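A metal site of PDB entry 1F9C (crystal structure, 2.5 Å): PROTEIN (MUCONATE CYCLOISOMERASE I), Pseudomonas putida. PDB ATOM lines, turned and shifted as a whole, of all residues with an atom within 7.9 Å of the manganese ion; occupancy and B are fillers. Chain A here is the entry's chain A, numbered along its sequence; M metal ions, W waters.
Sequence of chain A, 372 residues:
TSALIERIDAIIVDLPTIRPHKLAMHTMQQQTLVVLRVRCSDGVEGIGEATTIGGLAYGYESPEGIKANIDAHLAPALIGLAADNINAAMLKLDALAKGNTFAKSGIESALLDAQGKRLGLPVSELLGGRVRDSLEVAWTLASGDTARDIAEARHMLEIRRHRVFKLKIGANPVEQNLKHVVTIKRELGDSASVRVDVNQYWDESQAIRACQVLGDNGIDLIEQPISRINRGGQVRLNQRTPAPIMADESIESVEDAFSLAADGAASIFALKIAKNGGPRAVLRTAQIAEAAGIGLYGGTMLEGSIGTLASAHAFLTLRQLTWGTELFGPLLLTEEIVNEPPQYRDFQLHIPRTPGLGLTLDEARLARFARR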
ATOM      1  N   TYR A  58     -11.047  20.238  -1.713  1.00  0.00           N
ATOM      2  CA  TYR A  58     -11.808  20.109  -0.484  1.00  0.00           C
ATOM      3  C   TYR A  58     -13.325  20.217  -0.695  1.00  0.00           C
ATOM      4  O   TYR A  58     -14.095  20.243   0.263  1.00  0.00           O
ATOM      5  CB  TYR A  58     -11.361  21.187   0.506  1.00  0.00           C
ATOM      6  CG  TYR A  58     -10.161  20.811   1.348  1.00  0.00           C
ATOM      7  CD1 TYR A  58      -8.880  20.743   0.787  1.00  0.00           C
ATOM      8  CD2 TYR A  58     -10.300  20.537   2.707  1.00  0.00           C
ATOM      9  CE1 TYR A  58      -7.771  20.425   1.577  1.00  0.00           C
ATOM     10  CE2 TYR A  58      -9.206  20.212   3.501  1.00  0.00           C
ATOM     11  CZ  TYR A  58      -7.930  20.162   2.928  1.00  0.00           C
ATOM     12  OH  TYR A  58      -6.848  19.858   3.719  1.00  0.00           O
ATOM     13  N   LYS A 166      -5.639  21.122  17.003  1.00  0.00           N
ATOM     14  CA  LYS A 166      -5.882  19.988  16.149  1.00  0.00           C
ATOM     15  C   LYS A 166      -4.709  19.801  15.217  1.00  0.00           C
ATOM     16  O   LYS A 166      -4.060  20.766  14.797  1.00  0.00           O
ATOM     17  CB  LYS A 166      -7.179  20.149  15.354  1.00  0.00           C
ATOM     18  CG  LYS A 166      -7.393  21.503  14.745  1.00  0.00           C
ATOM     19  CD  LYS A 166      -8.674  21.532  13.912  1.00  0.00           C
ATOM     20  CE  LYS A 166      -8.774  20.324  12.986  1.00  0.00           C
ATOM     21  NZ  LYS A 166      -9.924  20.432  12.059  1.00  0.00           N
ATOM     22  N   LYS A 168      -3.511  18.116  11.613  1.00  0.00           N
ATOM     23  CA  LYS A 168      -3.953  17.587  10.326  1.00  0.00           C
ATOM     24  C   LYS A 168      -2.995  16.450   9.997  1.00  0.00           C
ATOM     25  O   LYS A 168      -1.808  16.671   9.756  1.00  0.00           O
ATOM     26  CB  LYS A 168      -3.867  18.660   9.242  1.00  0.00           C
ATOM     27  CG  LYS A 168      -4.879  19.781   9.406  1.00  0.00           C
ATOM     28  CD  LYS A 168      -5.486  20.169   8.064  1.00  0.00           C
ATOM     29  CE  LYS A 168      -4.439  20.730   7.098  1.00  0.00           C
ATOM     30  NZ  LYS A 168      -4.960  21.889   6.292  1.00  0.00           N
ATOM     31  N   VAL A 196      -7.501  15.398  16.207  1.00  0.00           N
ATOM     32  CA  VAL A 196      -6.914  15.182  14.891  1.00  0.00           C
ATOM     33  C   VAL A 196      -7.993  15.308  13.825  1.00  0.00           C
ATOM     34  O   VAL A 196      -9.182  15.216  14.101  1.00  0.00           O
ATOM     35  CB  VAL A 196      -6.241  13.785  14.727  1.00  0.00           C
ATOM     36  CG1 VAL A 196      -5.126  13.608  15.750  1.00  0.00           C
ATOM     37  CG2 VAL A 196      -7.277  12.680  14.827  1.00  0.00           C
ATOM     38  N   ASP A 197      -7.545  15.545  12.606  1.00  0.00           N
ATOM     39  CA  ASP A 197      -8.425  15.664  11.466  1.00  0.00           C
ATOM     40  C   ASP A 197      -7.653  14.916  10.384  1.00  0.00           C
ATOM     41  O   ASP A 197      -6.618  15.391   9.921  1.00  0.00           O
ATOM     42  CB  ASP A 197      -8.618  17.130  11.074  1.00  0.00           C
ATOM     43  CG  ASP A 197      -9.796  17.334  10.138  1.00  0.00           C
ATOM     44  OD1 ASP A 197     -10.177  16.381   9.421  1.00  0.00           O
ATOM     45  OD2 ASP A 197     -10.333  18.458  10.112  1.00  0.00           O
ATOM     46  N   VAL A 198      -8.126  13.743  10.023  1.00  0.00           N
ATOM     47  CA  VAL A 198      -7.429  12.967   9.016  1.00  0.00           C
ATOM     48  C   VAL A 198      -7.917  13.288   7.619  1.00  0.00           C
ATOM     49  O   VAL A 198      -7.387  12.776   6.638  1.00  0.00           O
ATOM     50  CB  VAL A 198      -7.563  11.449   9.253  1.00  0.00           C
ATOM     51  CG1 VAL A 198      -6.417  10.718   8.560  1.00  0.00           C
ATOM     52  CG2 VAL A 198      -7.558  11.147  10.743  1.00  0.00           C
ATOM     53  N   ASN A 199      -8.931  14.144   7.526  1.00  0.00           N
ATOM     54  CA  ASN A 199      -9.469  14.551   6.240  1.00  0.00           C
ATOM     55  C   ASN A 199      -9.703  13.419   5.234  1.00  0.00           C
ATOM     56  O   ASN A 199      -9.377  13.556   4.047  1.00  0.00           O
ATOM     57  CB  ASN A 199      -8.532  15.588   5.607  1.00  0.00           C
ATOM     58  CG  ASN A 199      -9.179  16.947   5.478  1.00  0.00           C
ATOM     59  OD1 ASN A 199      -9.959  17.185   4.545  1.00  0.00           O
ATOM     60  ND2 ASN A 199      -8.863  17.855   6.417  1.00  0.00           N
ATOM     61  N   GLN A 200     -10.270  12.310   5.698  1.00  0.00           N
ATOM     62  CA  GLN A 200     -10.568  11.146   4.857  1.00  0.00           C
ATOM     63  C   GLN A 200      -9.360  10.381   4.343  1.00  0.00           C
ATOM     64  O   GLN A 200      -9.508   9.448   3.554  1.00  0.00           O
ATOM     65  CB  GLN A 200     -11.416  11.571   3.662  1.00  0.00           C
ATOM     66  CG  GLN A 200     -12.787  12.104   4.022  1.00  0.00           C
ATOM     67  CD  GLN A 200     -13.599  12.499   2.814  1.00  0.00           C
ATOM     68  OE1 GLN A 200     -14.706  12.003   2.612  1.00  0.00           O
ATOM     69  NE2 GLN A 200     -13.057  13.394   2.014  1.00  0.00           N
ATOM     70  N   GLU A 223     -11.507  13.527  14.047  1.00  0.00           N
ATOM     71  CA  GLU A 223     -12.269  14.107  12.969  1.00  0.00           C
ATOM     72  C   GLU A 223     -12.056  13.446  11.605  1.00  0.00           C
ATOM     73  O   GLU A 223     -10.924  13.339  11.122  1.00  0.00           O
ATOM     74  CB  GLU A 223     -11.927  15.583  12.878  1.00  0.00           C
ATOM     75  CG  GLU A 223     -12.903  16.414  12.087  1.00  0.00           C
ATOM     76  CD  GLU A 223     -12.666  17.893  12.286  1.00  0.00           C
ATOM     77  OE1 GLU A 223     -11.891  18.263  13.190  1.00  0.00           O
ATOM     78  OE2 GLU A 223     -13.257  18.696  11.527  1.00  0.00           O
ATOM     79  N   GLN A 224     -13.160  12.988  11.008  1.00  0.00           N
ATOM     80  CA  GLN A 224     -13.169  12.342   9.698  1.00  0.00           C
ATOM     81  C   GLN A 224     -11.954  11.462   9.384  1.00  0.00           C
ATOM     82  O   GLN A 224     -11.205  11.717   8.434  1.00  0.00           O
ATOM     83  CB  GLN A 224     -13.306  13.397   8.602  1.00  0.00           C
ATOM     84  CG  GLN A 224     -13.703  12.842   7.254  1.00  0.00           C
ATOM     85  CD  GLN A 224     -15.185  12.567   7.154  1.00  0.00           C
ATOM     86  OE1 GLN A 224     -15.999  13.293   7.740  1.00  0.00           O
ATOM     87  NE2 GLN A 224     -15.556  11.522   6.418  1.00  0.00           N
ATOM     88  N   MET A 246     -15.883  12.245  14.695  1.00  0.00           N
ATOM     89  CA  MET A 246     -16.620  13.424  14.246  1.00  0.00           C
ATOM     90  C   MET A 246     -16.734  13.413  12.730  1.00  0.00           C
ATOM     91  O   MET A 246     -15.753  13.163  12.012  1.00  0.00           O
ATOM     92  CB  MET A 246     -15.919  14.721  14.684  1.00  0.00           C
ATOM     93  CG  MET A 246     -16.765  15.964  14.418  1.00  0.00           C
ATOM     94  SD  MET A 246     -15.848  17.518  14.247  1.00  0.00           S
ATOM     95  CE  MET A 246     -15.420  17.837  15.917  1.00  0.00           C
ATOM     96  N   ALA A 247     -17.933  13.692  12.233  1.00  0.00           N
ATOM     97  CA  ALA A 247     -18.159  13.723  10.800  1.00  0.00           C
ATOM     98  C   ALA A 247     -18.028  15.137  10.250  1.00  0.00           C
ATOM     99  O   ALA A 247     -18.637  16.081  10.775  1.00  0.00           O
ATOM    100  CB  ALA A 247     -19.539  13.168  10.474  1.00  0.00           C
ATOM    101  N   ASP A 248     -17.206  15.299   9.210  1.00  0.00           N
ATOM    102  CA  ASP A 248     -17.058  16.595   8.565  1.00  0.00           C
ATOM    103  C   ASP A 248     -17.337  16.445   7.078  1.00  0.00           C
ATOM    104  O   ASP A 248     -18.435  16.741   6.609  1.00  0.00           O
ATOM    105  CB  ASP A 248     -15.671  17.193   8.771  1.00  0.00           C
ATOM    106  CG  ASP A 248     -15.542  18.559   8.109  1.00  0.00           C
ATOM    107  OD1 ASP A 248     -16.541  18.996   7.495  1.00  0.00           O
ATOM    108  OD2 ASP A 248     -14.470  19.192   8.199  1.00  0.00           O
ATOM    109  N   GLU A 249     -16.343  15.968   6.321  1.00  0.00           N
ATOM    110  CA  GLU A 249     -16.518  15.798   4.880  1.00  0.00           C
ATOM    111  C   GLU A 249     -17.710  14.902   4.525  1.00  0.00           C
ATOM    112  O   GLU A 249     -18.253  15.002   3.432  1.00  0.00           O
ATOM    113  CB  GLU A 249     -15.245  15.209   4.248  1.00  0.00           C
ATOM    114  CG  GLU A 249     -14.168  16.236   3.961  1.00  0.00           C
ATOM    115  CD  GLU A 249     -13.539  16.775   5.224  1.00  0.00           C
ATOM    116  OE1 GLU A 249     -13.417  16.014   6.209  1.00  0.00           O
ATOM    117  OE2 GLU A 249     -13.162  17.970   5.229  1.00  0.00           O
ATOM    118  N   ALA A 270     -19.458  18.231  12.668  1.00  0.00           N
ATOM    119  CA  ALA A 270     -18.774  19.514  12.519  1.00  0.00           C
ATOM    120  C   ALA A 270     -19.804  20.361  11.786  1.00  0.00           C
ATOM    121  O   ALA A 270     -20.516  19.868  10.915  1.00  0.00           O
ATOM    122  CB  ALA A 270     -17.521  19.352  11.662  1.00  0.00           C
ATOM    123  N   LYS A 272     -20.361  23.416   9.320  1.00  0.00           N
ATOM    124  CA  LYS A 272     -19.781  24.353   8.373  1.00  0.00           C
ATOM    125  C   LYS A 272     -20.911  24.868   7.497  1.00  0.00           C
ATOM    126  O   LYS A 272     -21.594  24.090   6.836  1.00  0.00           O
ATOM    127  CB  LYS A 272     -18.724  23.661   7.506  1.00  0.00           C
ATOM    128  CG  LYS A 272     -17.494  23.240   8.258  1.00  0.00           C
ATOM    129  CD  LYS A 272     -16.426  22.712   7.315  1.00  0.00           C
ATOM    130  CE  LYS A 272     -15.207  22.212   8.080  1.00  0.00           C
ATOM    131  NZ  LYS A 272     -14.171  21.622   7.192  1.00  0.00           N
ATOM    132  N   TYR A 297     -19.832  21.000  16.828  1.00  0.00           N
ATOM    133  CA  TYR A 297     -18.534  21.626  16.667  1.00  0.00           C
ATOM    134  C   TYR A 297     -18.666  22.669  15.567  1.00  0.00           C
ATOM    135  O   TYR A 297     -19.223  22.386  14.496  1.00  0.00           O
ATOM    136  CB  TYR A 297     -17.515  20.556  16.276  1.00  0.00           C
ATOM    137  CG  TYR A 297     -16.107  21.033  15.997  1.00  0.00           C
ATOM    138  CD1 TYR A 297     -15.267  21.426  17.032  1.00  0.00           C
ATOM    139  CD2 TYR A 297     -15.595  21.025  14.707  1.00  0.00           C
ATOM    140  CE1 TYR A 297     -13.932  21.786  16.788  1.00  0.00           C
ATOM    141  CE2 TYR A 297     -14.264  21.381  14.449  1.00  0.00           C
ATOM    142  CZ  TYR A 297     -13.440  21.758  15.493  1.00  0.00           C
ATOM    143  OH  TYR A 297     -12.120  22.085  15.239  1.00  0.00           O
ATOM    144  N   GLY A 299     -17.368  24.311  12.649  1.00  0.00           N
ATOM    145  CA  GLY A 299     -16.329  24.109  11.650  1.00  0.00           C
ATOM    146  C   GLY A 299     -16.061  25.301  10.743  1.00  0.00           C
ATOM    147  O   GLY A 299     -16.821  26.266  10.726  1.00  0.00           O
ATOM    148  N   THR A 300     -14.987  25.212   9.972  1.00  0.00           N
ATOM    149  CA  THR A 300     -14.614  26.297   9.071  1.00  0.00           C
ATOM    150  C   THR A 300     -13.962  25.757   7.798  1.00  0.00           C
ATOM    151  O   THR A 300     -13.486  24.628   7.754  1.00  0.00           O
ATOM    152  CB  THR A 300     -13.624  27.262   9.775  1.00  0.00           C
ATOM    153  OG1 THR A 300     -13.458  28.442   8.982  1.00  0.00           O
ATOM    154  CG2 THR A 300     -12.258  26.605   9.965  1.00  0.00           C
ATOM    155  N   MET A 301     -13.966  26.579   6.756  1.00  0.00           N
ATOM    156  CA  MET A 301     -13.329  26.235   5.493  1.00  0.00           C
ATOM    157  C   MET A 301     -12.219  27.274   5.383  1.00  0.00           C
ATOM    158  O   MET A 301     -11.714  27.561   4.304  1.00  0.00           O
ATOM    159  CB  MET A 301     -14.286  26.395   4.318  1.00  0.00           C
ATOM    160  CG  MET A 301     -15.342  25.289   4.219  1.00  0.00           C
ATOM    161  SD  MET A 301     -14.656  23.604   4.148  1.00  0.00           S
ATOM    162  CE  MET A 301     -13.694  23.691   2.585  1.00  0.00           C
ATOM    163  N   GLU A 326     -13.589  25.916  15.453  1.00  0.00           N
ATOM    164  CA  GLU A 326     -12.279  26.072  14.870  1.00  0.00           C
ATOM    165  C   GLU A 326     -12.389  27.322  13.988  1.00  0.00           C
ATOM    166  O   GLU A 326     -11.858  27.355  12.892  1.00  0.00           O
ATOM    167  CB  GLU A 326     -11.905  24.859  14.022  1.00  0.00           C
ATOM    168  CG  GLU A 326     -12.960  24.461  13.014  1.00  0.00           C
ATOM    169  CD  GLU A 326     -12.568  23.230  12.213  1.00  0.00           C
ATOM    170  OE1 GLU A 326     -11.622  22.531  12.624  1.00  0.00           O
ATOM    171  OE2 GLU A 326     -13.207  22.956  11.170  1.00  0.00           O
HETATM  172 MN    MN M   1     -12.492  18.702   9.102  1.00  0.00          MN
HETATM  173  O   HOH W   1     -12.583  16.314   8.493  1.00  0.00           O
HETATM  174  O   HOH W   2     -12.132  21.114   9.374  1.00  0.00           O
HETATM  175  O   HOH W   3     -11.418  19.226   6.947  1.00  0.00           O
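The backbone NH of Asp 248 sits at hydrogen-bond distance from the side-chain amide oxygen of Gln 224 (2.8 Å). OE1 of Gln 224 is in hydrogen-bond range of N of Glu 249. The backbone NH (N) of Val 198 sits at hydrogen-bond distance from the backbone carbonyl oxygen (O) of Glu 223 (3.0 Å). The side-chain amino group of Lys 272 sits at hydrogen-bond distance from the side-chain sulfur of Met 301. NZ of Lys 272 lies within salt-bridge range of OD1 of Asp 248 (3.6 Å). The backbone carbonyl oxygen of Val 196 lies within hydrogen-bond range of the backbone NH of Glu 223 (2.9 Å). The side-chain carboxylate of Asp 197 sits close to the side-chain amino group of Lys 166 (2.8 Å). The side-chain amino group (NZ) of Lys 272 lies close to the backbone carbonyl oxygen (O) of Thr 300, 3.1 Å away.
Residues that only touch the manganese ion: Lys 272 (3.9 Å) and Glu 249 (3.998 Å). Of the 21 residues printed, 5 come within 4 Å of the manganese ion.
The manganese ion is bound by the side-chain carboxylate (OD2) of Asp 248 (2.2 Å), the side-chain carboxylate (OD2) of Asp 197 (2.4 Å), water W2 (2.5 Å), water W3 (2.5 Å), water W1 (2.5 Å) and the side-chain carboxylate (OE2) of Glu 223 (2.5 Å). The manganese ion has six donor atoms within binding distance.
Water W3 lies within hydrogen-bond range of the side-chain carboxylate (OE2) of Glu 249 (2.8 Å) and the side-chain amide nitrogen (ND2) of Asn 199 (2.9 Å). Water W1 bridges the side-chain carboxylate of Glu 249 and the side-chain carboxylate of Asp 197. Water W2 lies within hydrogen-bond range of the side-chain carboxylate of Glu 326 (2.8 Å) and the side-chain amino group of Lys 272 (3.0 Å).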
